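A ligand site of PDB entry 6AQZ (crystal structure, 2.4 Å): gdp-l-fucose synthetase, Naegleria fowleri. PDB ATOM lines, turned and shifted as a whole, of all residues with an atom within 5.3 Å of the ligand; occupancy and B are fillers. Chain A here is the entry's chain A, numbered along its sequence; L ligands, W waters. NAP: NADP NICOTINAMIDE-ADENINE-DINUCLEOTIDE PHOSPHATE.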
ATOM      1  N   GLY A  31       0.053 -25.272  23.077  1.00  0.00           N
ATOM      2  CA  GLY A  31       1.426 -24.886  22.788  1.00  0.00           C
ATOM      3  C   GLY A  31       2.434 -25.967  23.113  1.00  0.00           C
ATOM      4  O   GLY A  31       3.580 -25.662  23.479  1.00  0.00           O
ATOM      5  N   GLY A  32       2.027 -27.225  22.990  1.00  0.00           N
ATOM      6  CA  GLY A  32       2.898 -28.335  23.336  1.00  0.00           C
ATOM      7  C   GLY A  32       4.005 -28.662  22.339  1.00  0.00           C
ATOM      8  O   GLY A  32       4.797 -29.544  22.629  1.00  0.00           O
ATOM      9  N   THR A  33       4.048 -27.992  21.169  1.00  0.00           N
ATOM     10  CA  THR A  33       5.056 -28.234  20.151  1.00  0.00           C
ATOM     11  C   THR A  33       6.193 -27.220  20.174  1.00  0.00           C
ATOM     12  O   THR A  33       7.174 -27.394  19.445  1.00  0.00           O
ATOM     13  CB  THR A  33       4.440 -28.269  18.731  1.00  0.00           C
ATOM     14  OG1 THR A  33       3.818 -27.015  18.425  1.00  0.00           O
ATOM     15  CG2 THR A  33       3.389 -29.399  18.605  1.00  0.00           C
ATOM     16  N   GLY A  34       6.100 -26.175  21.009  1.00  0.00           N
ATOM     17  CA  GLY A  34       7.138 -25.176  21.103  1.00  0.00           C
ATOM     18  C   GLY A  34       8.212 -25.575  22.096  1.00  0.00           C
ATOM     19  O   GLY A  34       8.217 -26.678  22.647  1.00  0.00           O
ATOM     20  N   LEU A  35       9.086 -24.610  22.406  1.00  0.00           N
ATOM     21  CA  LEU A  35      10.201 -24.872  23.309  1.00  0.00           C
ATOM     22  C   LEU A  35       9.758 -25.485  24.644  1.00  0.00           C
ATOM     23  O   LEU A  35      10.134 -26.616  24.994  1.00  0.00           O
ATOM     24  CB  LEU A  35      10.971 -23.566  23.531  1.00  0.00           C
ATOM     25  CG  LEU A  35      12.028 -23.624  24.622  1.00  0.00           C
ATOM     26  CD1 LEU A  35      13.147 -24.590  24.193  1.00  0.00           C
ATOM     27  CD2 LEU A  35      12.594 -22.260  24.911  1.00  0.00           C
ATOM     28  N   PHE A  36       8.925 -24.763  25.402  1.00  0.00           N
ATOM     29  CA  PHE A  36       8.517 -25.215  26.736  1.00  0.00           C
ATOM     30  C   PHE A  36       7.729 -26.524  26.635  1.00  0.00           C
ATOM     31  O   PHE A  36       7.985 -27.479  27.384  1.00  0.00           O
ATOM     32  CB  PHE A  36       7.683 -24.109  27.424  1.00  0.00           C
ATOM     33  CG  PHE A  36       7.695 -24.141  28.961  1.00  0.00           C
ATOM     34  CD1 PHE A  36       8.292 -25.191  29.665  1.00  0.00           C
ATOM     35  CD2 PHE A  36       7.087 -23.126  29.678  1.00  0.00           C
ATOM     36  CE1 PHE A  36       8.277 -25.212  31.047  1.00  0.00           C
ATOM     37  CE2 PHE A  36       7.078 -23.130  31.092  1.00  0.00           C
ATOM     38  CZ  PHE A  36       7.662 -24.175  31.766  1.00  0.00           C
ATOM     39  N   GLY A  37       6.830 -26.605  25.651  1.00  0.00           N
ATOM     40  CA  GLY A  37       5.994 -27.792  25.517  1.00  0.00           C
ATOM     41  C   GLY A  37       6.790 -29.063  25.249  1.00  0.00           C
ATOM     42  O   GLY A  37       6.488 -30.116  25.834  1.00  0.00           O
ATOM     43  N   LEU A  56      -0.740 -30.269  21.875  1.00  0.00           N
ATOM     44  CA  LEU A  56      -1.398 -29.595  20.767  1.00  0.00           C
ATOM     45  C   LEU A  56      -0.445 -28.630  20.077  1.00  0.00           C
ATOM     46  O   LEU A  56       0.396 -27.990  20.717  1.00  0.00           O
ATOM     47  CB  LEU A  56      -2.604 -28.786  21.259  1.00  0.00           C
ATOM     48  CG  LEU A  56      -3.790 -29.465  21.961  1.00  0.00           C
ATOM     49  CD1 LEU A  56      -4.715 -28.378  22.404  1.00  0.00           C
ATOM     50  CD2 LEU A  56      -4.512 -30.408  21.034  1.00  0.00           C
ATOM     51  N   GLY A  57      -0.626 -28.471  18.775  1.00  0.00           N
ATOM     52  CA  GLY A  57      -0.016 -27.374  18.058  1.00  0.00           C
ATOM     53  C   GLY A  57      -1.067 -26.664  17.220  1.00  0.00           C
ATOM     54  O   GLY A  57      -2.209 -27.106  17.127  1.00  0.00           O
ATOM     55  N   SER A  58      -0.634 -25.598  16.581  1.00  0.00           N
ATOM     56  CA  SER A  58      -1.533 -24.839  15.719  1.00  0.00           C
ATOM     57  C   SER A  58      -2.103 -25.709  14.603  1.00  0.00           C
ATOM     58  O   SER A  58      -3.220 -25.455  14.128  1.00  0.00           O
ATOM     59  CB  SER A  58      -0.811 -23.619  15.142  1.00  0.00           C
ATOM     60  OG  SER A  58       0.360 -24.005  14.455  1.00  0.00           O
ATOM     61  N   LYS A  59      -1.349 -26.711  14.129  1.00  0.00           N
ATOM     62  CA  LYS A  59      -1.895 -27.620  13.115  1.00  0.00           C
ATOM     63  C   LYS A  59      -3.145 -28.336  13.627  1.00  0.00           C
ATOM     64  O   LYS A  59      -4.018 -28.701  12.831  1.00  0.00           O
ATOM     65  CB  LYS A  59      -0.844 -28.637  12.643  1.00  0.00           C
ATOM     66  N   GLY A  61      -5.462 -26.930  15.395  1.00  0.00           N
ATOM     67  CA  GLY A  61      -6.551 -25.980  15.461  1.00  0.00           C
ATOM     68  C   GLY A  61      -6.131 -24.639  16.029  1.00  0.00           C
ATOM     69  O   GLY A  61      -5.316 -24.594  16.959  1.00  0.00           O
ATOM     70  N   ASP A  62      -6.656 -23.544  15.471  1.00  0.00           N
ATOM     71  CA  ASP A  62      -6.311 -22.174  15.821  1.00  0.00           C
ATOM     72  C   ASP A  62      -7.048 -21.778  17.109  1.00  0.00           C
ATOM     73  O   ASP A  62      -8.240 -21.461  17.072  1.00  0.00           O
ATOM     74  CB  ASP A  62      -6.645 -21.258  14.643  1.00  0.00           C
ATOM     75  CG  ASP A  62      -6.357 -19.769  14.924  1.00  0.00           C
ATOM     76  OD1 ASP A  62      -5.782 -19.408  15.982  1.00  0.00           O
ATOM     77  OD2 ASP A  62      -6.733 -18.943  14.057  1.00  0.00           O
ATOM     78  N   LEU A  63      -6.329 -21.750  18.240  1.00  0.00           N
ATOM     79  CA  LEU A  63      -6.950 -21.496  19.547  1.00  0.00           C
ATOM     80  C   LEU A  63      -7.443 -20.056  19.716  1.00  0.00           C
ATOM     81  O   LEU A  63      -8.052 -19.750  20.753  1.00  0.00           O
ATOM     82  CB  LEU A  63      -5.996 -21.872  20.675  1.00  0.00           C
ATOM     83  CG  LEU A  63      -5.477 -23.323  20.625  1.00  0.00           C
ATOM     84  CD1 LEU A  63      -4.426 -23.569  21.695  1.00  0.00           C
ATOM     85  CD2 LEU A  63      -6.608 -24.346  20.762  1.00  0.00           C
ATOM     86  N   ARG A  64      -7.183 -19.161  18.763  1.00  0.00           N
ATOM     87  CA  ARG A  64      -7.769 -17.834  18.820  1.00  0.00           C
ATOM     88  C   ARG A  64      -9.242 -17.849  18.476  1.00  0.00           C
ATOM     89  O   ARG A  64      -9.979 -16.940  18.876  1.00  0.00           O
ATOM     90  CB  ARG A  64      -7.034 -16.886  17.864  1.00  0.00           C
ATOM     91  CG  ARG A  64      -5.619 -16.605  18.269  1.00  0.00           C
ATOM     92  CD  ARG A  64      -4.847 -15.927  17.159  1.00  0.00           C
ATOM     93  NE  ARG A  64      -4.655 -16.831  16.034  1.00  0.00           N
ATOM     94  CZ  ARG A  64      -4.095 -16.489  14.887  1.00  0.00           C
ATOM     95  NH1 ARG A  64      -3.659 -15.241  14.709  1.00  0.00           N
ATOM     96  NH2 ARG A  64      -3.942 -17.396  13.912  1.00  0.00           N
ATOM     97  N   HIS A  83      -1.448 -24.702  29.911  1.00  0.00           N
ATOM     98  CA  HIS A  83      -1.725 -23.728  28.854  1.00  0.00           C
ATOM     99  C   HIS A  83      -0.433 -22.970  28.552  1.00  0.00           C
ATOM    100  O   HIS A  83      -0.079 -22.028  29.254  1.00  0.00           O
ATOM    101  CB  HIS A  83      -2.846 -22.790  29.303  1.00  0.00           C
ATOM    102  CG  HIS A  83      -3.055 -21.618  28.405  1.00  0.00           C
ATOM    103  ND1 HIS A  83      -3.005 -21.714  27.026  1.00  0.00           N
ATOM    104  CD2 HIS A  83      -3.385 -20.332  28.683  1.00  0.00           C
ATOM    105  CE1 HIS A  83      -3.242 -20.533  26.500  1.00  0.00           C
ATOM    106  NE2 HIS A  83      -3.497 -19.671  27.479  1.00  0.00           N
ATOM    107  N   LEU A  84       0.293 -23.421  27.520  1.00  0.00           N
ATOM    108  CA  LEU A  84       1.533 -22.772  27.100  1.00  0.00           C
ATOM    109  C   LEU A  84       1.384 -21.992  25.799  1.00  0.00           C
ATOM    110  O   LEU A  84       2.252 -21.176  25.488  1.00  0.00           O
ATOM    111  CB  LEU A  84       2.649 -23.818  26.932  1.00  0.00           C
ATOM    112  CG  LEU A  84       2.932 -24.770  28.122  1.00  0.00           C
ATOM    113  CD1 LEU A  84       4.015 -25.789  27.737  1.00  0.00           C
ATOM    114  CD2 LEU A  84       3.317 -24.080  29.402  1.00  0.00           C
ATOM    115  N   ALA A  85       0.329 -22.201  25.042  1.00  0.00           N
ATOM    116  CA  ALA A  85       0.212 -21.527  23.763  1.00  0.00           C
ATOM    117  C   ALA A  85       0.128 -20.023  23.974  1.00  0.00           C
ATOM    118  O   ALA A  85      -0.504 -19.538  24.924  1.00  0.00           O
ATOM    119  CB  ALA A  85      -1.044 -22.005  23.023  1.00  0.00           C
ATOM    120  N   ALA A  86       0.813 -19.284  23.100  1.00  0.00           N
ATOM    121  CA  ALA A  86       0.784 -17.833  23.085  1.00  0.00           C
ATOM    122  C   ALA A  86       1.189 -17.373  21.685  1.00  0.00           C
ATOM    123  O   ALA A  86       1.890 -18.074  20.968  1.00  0.00           O
ATOM    124  CB  ALA A  86       1.713 -17.226  24.118  1.00  0.00           C
ATOM    125  N   PHE A  87       0.798 -16.159  21.355  1.00  0.00           N
ATOM    126  CA  PHE A  87       1.242 -15.540  20.119  1.00  0.00           C
ATOM    127  C   PHE A  87       2.390 -14.618  20.478  1.00  0.00           C
ATOM    128  O   PHE A  87       2.212 -13.609  21.150  1.00  0.00           O
ATOM    129  CB  PHE A  87       0.109 -14.793  19.429  1.00  0.00           C
ATOM    130  CG  PHE A  87       0.561 -13.992  18.259  1.00  0.00           C
ATOM    131  CD1 PHE A  87       0.872 -14.599  17.080  1.00  0.00           C
ATOM    132  CD2 PHE A  87       0.668 -12.604  18.356  1.00  0.00           C
ATOM    133  CE1 PHE A  87       1.301 -13.854  15.999  1.00  0.00           C
ATOM    134  CE2 PHE A  87       1.094 -11.851  17.281  1.00  0.00           C
ATOM    135  CZ  PHE A  87       1.412 -12.480  16.099  1.00  0.00           C
ATOM    136  N   VAL A  88       3.598 -15.009  20.069  1.00  0.00           N
ATOM    137  CA  VAL A  88       4.827 -14.352  20.484  1.00  0.00           C
ATOM    138  C   VAL A  88       5.429 -13.563  19.359  1.00  0.00           C
ATOM    139  O   VAL A  88       6.492 -12.956  19.524  1.00  0.00           O
ATOM    140  CB  VAL A  88       5.842 -15.377  21.021  1.00  0.00           C
ATOM    141  CG1 VAL A  88       5.285 -16.069  22.223  1.00  0.00           C
ATOM    142  CG2 VAL A  88       6.212 -16.381  19.953  1.00  0.00           C
ATOM    143  N   MET A 108      -7.114 -16.005  22.564  1.00  0.00           N
ATOM    144  CA  MET A 108      -6.652 -17.354  22.903  1.00  0.00           C
ATOM    145  C   MET A 108      -6.771 -17.614  24.406  1.00  0.00           C
ATOM    146  O   MET A 108      -7.248 -18.680  24.827  1.00  0.00           O
ATOM    147  CB  MET A 108      -5.228 -17.498  22.353  1.00  0.00           C
ATOM    148  CG  MET A 108      -4.329 -18.553  22.884  1.00  0.00           C
ATOM    149  SD  MET A 108      -2.856 -18.881  21.860  1.00  0.00           S
ATOM    150  CE  MET A 108      -2.464 -17.419  20.902  1.00  0.00           C
ATOM    151  N   CYS A 127       0.845 -19.702  31.613  1.00  0.00           N
ATOM    152  CA  CYS A 127       2.238 -19.266  31.603  1.00  0.00           C
ATOM    153  C   CYS A 127       2.305 -17.761  31.387  1.00  0.00           C
ATOM    154  O   CYS A 127       1.761 -17.252  30.403  1.00  0.00           O
ATOM    155  CB  CYS A 127       2.998 -20.040  30.528  1.00  0.00           C
ATOM    156  SG  CYS A 127       4.726 -19.946  30.702  1.00  0.00           S
ATOM    157  N   LEU A 128       2.961 -17.052  32.300  1.00  0.00           N
ATOM    158  CA  LEU A 128       3.273 -15.629  32.162  1.00  0.00           C
ATOM    159  C   LEU A 128       4.749 -15.485  31.760  1.00  0.00           C
ATOM    160  O   LEU A 128       5.355 -16.416  31.228  1.00  0.00           O
ATOM    161  CB  LEU A 128       2.979 -14.862  33.462  1.00  0.00           C
ATOM    162  CG  LEU A 128       1.648 -15.127  34.155  1.00  0.00           C
ATOM    163  CD1 LEU A 128       1.448 -14.193  35.360  1.00  0.00           C
ATOM    164  CD2 LEU A 128       0.489 -15.067  33.218  1.00  0.00           C
ATOM    165  N   SER A 129       5.333 -14.321  32.038  1.00  0.00           N
ATOM    166  CA  SER A 129       6.709 -14.054  31.650  1.00  0.00           C
ATOM    167  C   SER A 129       7.243 -12.906  32.493  1.00  0.00           C
ATOM    168  O   SER A 129       6.471 -12.019  32.910  1.00  0.00           O
ATOM    169  CB  SER A 129       6.808 -13.730  30.155  1.00  0.00           C
ATOM    170  OG  SER A 129       7.259 -12.425  29.938  1.00  0.00           O
ATOM    171  N   THR A 130       8.549 -12.930  32.787  1.00  0.00           N
ATOM    172  CA  THR A 130       9.099 -11.868  33.633  1.00  0.00           C
ATOM    173  C   THR A 130       9.186 -10.523  32.916  1.00  0.00           C
ATOM    174  O   THR A 130       9.490  -9.523  33.568  1.00  0.00           O
ATOM    175  CB  THR A 130      10.484 -12.211  34.189  1.00  0.00           C
ATOM    176  OG1 THR A 130      11.440 -12.280  33.134  1.00  0.00           O
ATOM    177  CG2 THR A 130      10.459 -13.514  34.944  1.00  0.00           C
ATOM    178  N   TYR A 158       1.503  -7.367  24.513  1.00  0.00           N
ATOM    179  CA  TYR A 158       1.786  -8.702  24.993  1.00  0.00           C
ATOM    180  C   TYR A 158       1.765  -8.730  26.527  1.00  0.00           C
ATOM    181  O   TYR A 158       1.162  -9.613  27.137  1.00  0.00           O
ATOM    182  CB  TYR A 158       3.137  -9.158  24.429  1.00  0.00           C
ATOM    183  CG  TYR A 158       3.600 -10.503  24.890  1.00  0.00           C
ATOM    184  CD1 TYR A 158       3.193 -11.650  24.226  1.00  0.00           C
ATOM    185  CD2 TYR A 158       4.460 -10.638  25.973  1.00  0.00           C
ATOM    186  CE1 TYR A 158       3.626 -12.900  24.609  1.00  0.00           C
ATOM    187  CE2 TYR A 158       4.907 -11.896  26.372  1.00  0.00           C
ATOM    188  CZ  TYR A 158       4.472 -13.019  25.681  1.00  0.00           C
ATOM    189  OH  TYR A 158       4.875 -14.275  26.042  1.00  0.00           O
ATOM    190  N   LYS A 162      -0.872 -10.917  29.058  1.00  0.00           N
ATOM    191  CA  LYS A 162      -0.439 -11.856  30.093  1.00  0.00           C
ATOM    192  C   LYS A 162      -1.039 -11.494  31.452  1.00  0.00           C
ATOM    193  O   LYS A 162      -1.496 -12.370  32.204  1.00  0.00           O
ATOM    194  CB  LYS A 162       1.089 -11.932  30.177  1.00  0.00           C
ATOM    195  CG  LYS A 162       1.754 -12.602  29.019  1.00  0.00           C
ATOM    196  CD  LYS A 162       1.223 -14.010  28.827  1.00  0.00           C
ATOM    197  CE  LYS A 162       2.198 -14.930  28.036  1.00  0.00           C
ATOM    198  NZ  LYS A 162       1.467 -16.262  27.812  1.00  0.00           N
ATOM    199  N   PRO A 190       8.028 -18.157  34.024  1.00  0.00           N
ATOM    200  CA  PRO A 190       9.400 -18.568  33.712  1.00  0.00           C
ATOM    201  C   PRO A 190      10.211 -17.358  33.278  1.00  0.00           C
ATOM    202  O   PRO A 190       9.697 -16.370  32.770  1.00  0.00           O
ATOM    203  CB  PRO A 190       9.233 -19.594  32.595  1.00  0.00           C
ATOM    204  CG  PRO A 190       7.932 -19.257  31.957  1.00  0.00           C
ATOM    205  CD  PRO A 190       7.068 -18.625  33.013  1.00  0.00           C
ATOM    206  N   THR A 191      11.494 -17.447  33.548  1.00  0.00           N
ATOM    207  CA  THR A 191      12.480 -16.474  33.096  1.00  0.00           C
ATOM    208  C   THR A 191      12.929 -16.856  31.684  1.00  0.00           C
ATOM    209  O   THR A 191      12.189 -17.523  30.946  1.00  0.00           O
ATOM    210  CB  THR A 191      13.655 -16.443  34.088  1.00  0.00           C
ATOM    211  OG1 THR A 191      14.384 -15.228  33.937  1.00  0.00           O
ATOM    212  CG2 THR A 191      14.591 -17.694  33.887  1.00  0.00           C
ATOM    213  N   ASN A 192      14.080 -16.366  31.241  1.00  0.00           N
ATOM    214  CA  ASN A 192      14.651 -16.731  29.947  1.00  0.00           C
ATOM    215  C   ASN A 192      14.869 -18.227  29.798  1.00  0.00           C
ATOM    216  O   ASN A 192      15.743 -18.811  30.451  1.00  0.00           O
ATOM    217  CB  ASN A 192      15.975 -16.004  29.739  1.00  0.00           C
ATOM    218  CG  ASN A 192      15.845 -14.516  29.972  1.00  0.00           C
ATOM    219  OD1 ASN A 192      15.273 -13.798  29.162  1.00  0.00           O
ATOM    220  ND2 ASN A 192      16.328 -14.049  31.128  1.00  0.00           N
ATOM    221  N   LEU A 193      14.087 -18.864  28.944  1.00  0.00           N
ATOM    222  CA  LEU A 193      14.217 -20.283  28.683  1.00  0.00           C
ATOM    223  C   LEU A 193      15.165 -20.542  27.522  1.00  0.00           C
ATOM    224  O   LEU A 193      15.328 -19.702  26.626  1.00  0.00           O
ATOM    225  CB  LEU A 193      12.842 -20.899  28.383  1.00  0.00           C
ATOM    226  CG  LEU A 193      11.752 -20.801  29.447  1.00  0.00           C
ATOM    227  CD1 LEU A 193      10.526 -21.639  29.061  1.00  0.00           C
ATOM    228  CD2 LEU A 193      12.282 -21.139  30.830  1.00  0.00           C
ATOM    229  N   HIS A 197      14.345 -27.545  20.416  1.00  0.00           N
ATOM    230  CA  HIS A 197      13.099 -27.148  19.769  1.00  0.00           C
ATOM    231  C   HIS A 197      12.773 -25.672  19.939  1.00  0.00           C
ATOM    232  O   HIS A 197      11.635 -25.268  19.706  1.00  0.00           O
ATOM    233  CB  HIS A 197      11.934 -28.009  20.256  1.00  0.00           C
ATOM    234  CG  HIS A 197      12.104 -29.459  19.967  1.00  0.00           C
ATOM    235  ND1 HIS A 197      11.843 -30.004  18.728  1.00  0.00           N
ATOM    236  CD2 HIS A 197      12.507 -30.482  20.750  1.00  0.00           C
ATOM    237  CE1 HIS A 197      12.066 -31.301  18.764  1.00  0.00           C
ATOM    238  NE2 HIS A 197      12.472 -31.621  19.979  1.00  0.00           N
ATOM    239  N   HIS A 206      15.174 -15.598  20.488  1.00  0.00           N
ATOM    240  CA  HIS A 206      15.776 -15.110  21.717  1.00  0.00           C
ATOM    241  C   HIS A 206      17.289 -15.076  21.597  1.00  0.00           C
ATOM    242  O   HIS A 206      17.887 -15.718  20.734  1.00  0.00           O
ATOM    243  CB  HIS A 206      15.380 -15.990  22.898  1.00  0.00           C
ATOM    244  CG  HIS A 206      13.912 -16.028  23.150  1.00  0.00           C
ATOM    245  ND1 HIS A 206      13.100 -14.935  22.926  1.00  0.00           N
ATOM    246  CD2 HIS A 206      13.100 -17.024  23.600  1.00  0.00           C
ATOM    247  CE1 HIS A 206      11.845 -15.262  23.216  1.00  0.00           C
ATOM    248  NE2 HIS A 206      11.820 -16.516  23.629  1.00  0.00           N
ATOM    249  N   ARG A 340      13.780 -25.004  14.035  1.00  0.00           N
ATOM    250  CA  ARG A 340      13.120 -23.726  13.752  1.00  0.00           C
ATOM    251  C   ARG A 340      14.170 -22.644  13.549  1.00  0.00           C
ATOM    252  O   ARG A 340      14.932 -22.317  14.463  1.00  0.00           O
ATOM    253  CB  ARG A 340      12.205 -23.369  14.932  1.00  0.00           C
ATOM    254  CG  ARG A 340      10.969 -24.253  15.023  1.00  0.00           C
ATOM    255  CD  ARG A 340      10.250 -24.124  16.344  1.00  0.00           C
ATOM    256  NE  ARG A 340       9.651 -22.814  16.584  1.00  0.00           N
ATOM    257  CZ  ARG A 340       9.360 -22.342  17.805  1.00  0.00           C
ATOM    258  NH1 ARG A 340       9.631 -23.089  18.874  1.00  0.00           N
ATOM    259  NH2 ARG A 340       8.804 -21.145  17.954  1.00  0.00           N
HETATM  260  PA  NAP L   1       7.174 -21.223  21.273  1.00  0.00           P
HETATM  261  O1A NAP L   1       7.135 -20.062  20.334  1.00  0.00           O
HETATM  262  O2A NAP L   1       8.400 -22.097  21.408  1.00  0.00           O
HETATM  263  O5B NAP L   1       5.898 -22.236  21.027  1.00  0.00           O
HETATM  264  C5B NAP L   1       4.745 -21.513  21.287  1.00  0.00           C
HETATM  265  C4B NAP L   1       3.557 -22.504  21.120  1.00  0.00           C
HETATM  266  O4B NAP L   1       2.307 -21.792  20.937  1.00  0.00           O
HETATM  267  C3B NAP L   1       3.779 -23.475  19.886  1.00  0.00           C
HETATM  268  O3B NAP L   1       3.291 -24.756  20.198  1.00  0.00           O
HETATM  269  C2B NAP L   1       2.794 -22.890  18.860  1.00  0.00           C
HETATM  270  O2B NAP L   1       2.232 -23.803  18.064  1.00  0.00           O
HETATM  271  C1B NAP L   1       1.655 -22.457  19.871  1.00  0.00           C
HETATM  272  N9A NAP L   1       0.696 -21.553  19.245  1.00  0.00           N
HETATM  273  C8A NAP L   1       0.902 -20.241  18.878  1.00  0.00           C
HETATM  274  N7A NAP L   1      -0.188 -19.664  18.325  1.00  0.00           N
HETATM  275  C5A NAP L   1      -1.142 -20.657  18.349  1.00  0.00           C
HETATM  276  C6A NAP L   1      -2.471 -20.670  17.917  1.00  0.00           C
HETATM  277  N6A NAP L   1      -3.042 -19.528  17.362  1.00  0.00           N
HETATM  278  N1A NAP L   1      -3.243 -21.779  18.059  1.00  0.00           N
HETATM  279  C2A NAP L   1      -2.601 -22.844  18.624  1.00  0.00           C
HETATM  280  N3A NAP L   1      -1.339 -22.991  19.077  1.00  0.00           N
HETATM  281  C4A NAP L   1      -0.618 -21.854  18.928  1.00  0.00           C
HETATM  282  O3  NAP L   1       6.868 -20.411  22.700  1.00  0.00           O
HETATM  283  PN  NAP L   1       7.582 -21.056  23.971  1.00  0.00           P
HETATM  284  O1N NAP L   1       7.273 -22.486  24.176  1.00  0.00           O
HETATM  285  O2N NAP L   1       8.942 -20.461  24.261  1.00  0.00           O
HETATM  286  O5D NAP L   1       6.706 -20.336  25.312  1.00  0.00           O
HETATM  287  C5D NAP L   1       5.472 -20.909  25.515  1.00  0.00           C
HETATM  288  C4D NAP L   1       4.956 -20.209  26.745  1.00  0.00           C
HETATM  289  O4D NAP L   1       6.081 -19.915  27.589  1.00  0.00           O
HETATM  290  C3D NAP L   1       4.346 -18.792  26.300  1.00  0.00           C
HETATM  291  O3D NAP L   1       3.178 -18.553  27.001  1.00  0.00           O
HETATM  292  C2D NAP L   1       5.465 -17.806  26.681  1.00  0.00           C
HETATM  293  O2D NAP L   1       5.009 -16.578  27.117  1.00  0.00           O
HETATM  294  C1D NAP L   1       6.088 -18.534  27.907  1.00  0.00           C
HETATM  295  N1N NAP L   1       7.471 -18.013  28.169  1.00  0.00           N
HETATM  296  C2N NAP L   1       8.550 -18.343  27.345  1.00  0.00           C
HETATM  297  C3N NAP L   1       9.803 -17.809  27.605  1.00  0.00           C
HETATM  298  C7N NAP L   1      10.951 -18.165  26.703  1.00  0.00           C
HETATM  299  O7N NAP L   1      12.073 -17.653  26.832  1.00  0.00           O
HETATM  300  N7N NAP L   1      10.755 -19.090  25.679  1.00  0.00           N
HETATM  301  C4N NAP L   1      10.055 -16.891  28.733  1.00  0.00           C
HETATM  302  C5N NAP L   1       8.837 -16.585  29.534  1.00  0.00           C
HETATM  303  C6N NAP L   1       7.648 -17.126  29.256  1.00  0.00           C
HETATM  304  P2B NAP L   1       3.127 -24.184  16.476  1.00  0.00           P
HETATM  305  O1X NAP L   1       4.340 -24.858  17.040  1.00  0.00           O
HETATM  306  O2X NAP L   1       2.081 -25.080  15.813  1.00  0.00           O
HETATM  307  O3X NAP L   1       3.289 -22.802  15.936  1.00  0.00           O
HETATM  308  O   HOH W   1      -1.608 -25.327  20.503  1.00  0.00           O
HETATM  309  O   HOH W   2       1.287 -27.221  14.673  1.00  0.00           O
HETATM  310  O   HOH W   3       7.642 -14.535  26.405  1.00  0.00           O
HETATM  311  O   HOH W   4       9.443 -18.203  20.675  1.00  0.00           O
HETATM  312  O   HOH W   5      -1.384 -17.359  17.468  1.00  0.00           O
HETATM  313  O   HOH W   6       5.462 -21.774  16.464  1.00  0.00           O
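A nitrogen (N6A) of the ligand lies close to the guanidinium group (NE) of Arg 64. N of Gly 32 touches O3B of the ligand, 3.9 Å away. C of Gly 57 touches O2X of the ligand, 3.8 Å away. O of Gly 61 touches C2A of the ligand (3.6 Å). CA of Ala 85 touches O4B of the ligand, 3.5 Å away. Ala 86 touches the ligand. CG2 of Val 88 touches O1A of the ligand (3.8 Å). Leu 128 touches the ligand. Ser 129 touches the ligand (CB to C5N, 3.6 Å). Pro 190 touches the ligand. Thr 191 touches the ligand. Hydrophobic or aromatic side chains within 4 Å of the ligand: Leu 35, Phe 36, Leu 63, Ala 85, Ala 86, Val 88, Tyr 158, Pro 190, Leu 193 and His 206. Within 4 Å of the ligand: Gly 31, Gly 32, Thr 33, Gly 34, Leu 35, Phe 36, Gly 57, Ser 58, Gly 61, Asp 62, Leu 63, Arg 64, Leu 84, Ala 85, Ala 86, Val 88, Cys 127, Leu 128, Ser 129, Tyr 158, Lys 162, Pro 190, Thr 191, Leu 193, His 206 and Arg 340. The nearest printed residue that does not touch the ligand is Met 108 (4.1 Å).
The side-chain amino group of Lys 162 lies within hydrogen-bond range of the backbone carbonyl oxygen of Cys 127. The backbone carbonyl oxygen (O) of His 197 sits at hydrogen-bond distance from the guanidinium group (NH1) of Arg 340 (3.1 Å). OD1 of Asp 62 lies within salt-bridge range of NE of Arg 64 (2.8 Å). O of His 83 is in hydrogen-bond range of N of Cys 127. The backbone NH (N) of Gly 32 sits at hydrogen-bond distance from the backbone carbonyl oxygen (O) of Leu 56 (2.9 Å).
Water W2 lies within hydrogen-bond range of an oxygen (O2X) of the ligand, the backbone NH of Lys 59 and the backbone NH of Ser 58. Water W1 lies within hydrogen-bond range of N3A of the ligand (2.8 Å), N of Gly 31 (3.1 Å) and O of Leu 56 (3.3 Å). Water W3 lies within hydrogen-bond range of OH of Tyr 158 (2.8 Å) and O2D of the ligand (3.4 Å).
The backbone NH (N) of Ser 58 sits at hydrogen-bond distance from an oxygen (O2X) of the ligand, at 2.9 Å. The side-chain hydroxyl (OG) of Ser 58 is in hydrogen-bond range of an oxygen (O2X) of the ligand (2.4 Å). OH of Tyr 158 is in hydrogen-bond range of O2D of the ligand (2.5 Å). N of Thr 33 lies within hydrogen-bond range of O3B of the ligand (3.5 Å). The side-chain hydroxyl of Thr 33 lies within hydrogen-bond range of an oxygen (O1X) of the ligand, at 2.6 Å. N of Leu 35 lies within hydrogen-bond range of O2A of the ligand, at 2.8 Å. NZ of Lys 162 sits at hydrogen-bond distance from O3D of the ligand, at 3.0 Å. NH1 of Arg 340 lies within salt-bridge range of O2A of the ligand (3.0 Å). An oxygen (O1N) of the ligand lies within hydrogen-bond range of the backbone NH (N) of Phe 36 (3.1 Å). A nitrogen (N6A) of the ligand lies within hydrogen-bond range of the side-chain carboxylate (OD1) of Asp 62, at 3.1 Å. The backbone NH (N) of Leu 63 is in hydrogen-bond range of a nitrogen (N1A) of the ligand (3.1 Å). The backbone carbonyl oxygen (O) of Leu 84 sits close to an oxygen (O3D) of the ligand. An oxygen (O7N) of the ligand sits at hydrogen-bond distance from the backbone NH (N) of Leu 193 (3.2 Å). An oxygen (O3B) of the ligand sits at hydrogen-bond distance from the backbone NH (N) of Gly 34 (3.2 Å). An oxygen (O3B) of the ligand lies close to the backbone carbonyl oxygen (O) of Gly 31. An oxygen (O4D) of the ligand lies within hydrogen-bond range of the side-chain sulfur of Cys 127 (3.4 Å). NE2 of His 206 sits at hydrogen-bond distance from O7N of the ligand (3.4 Å).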
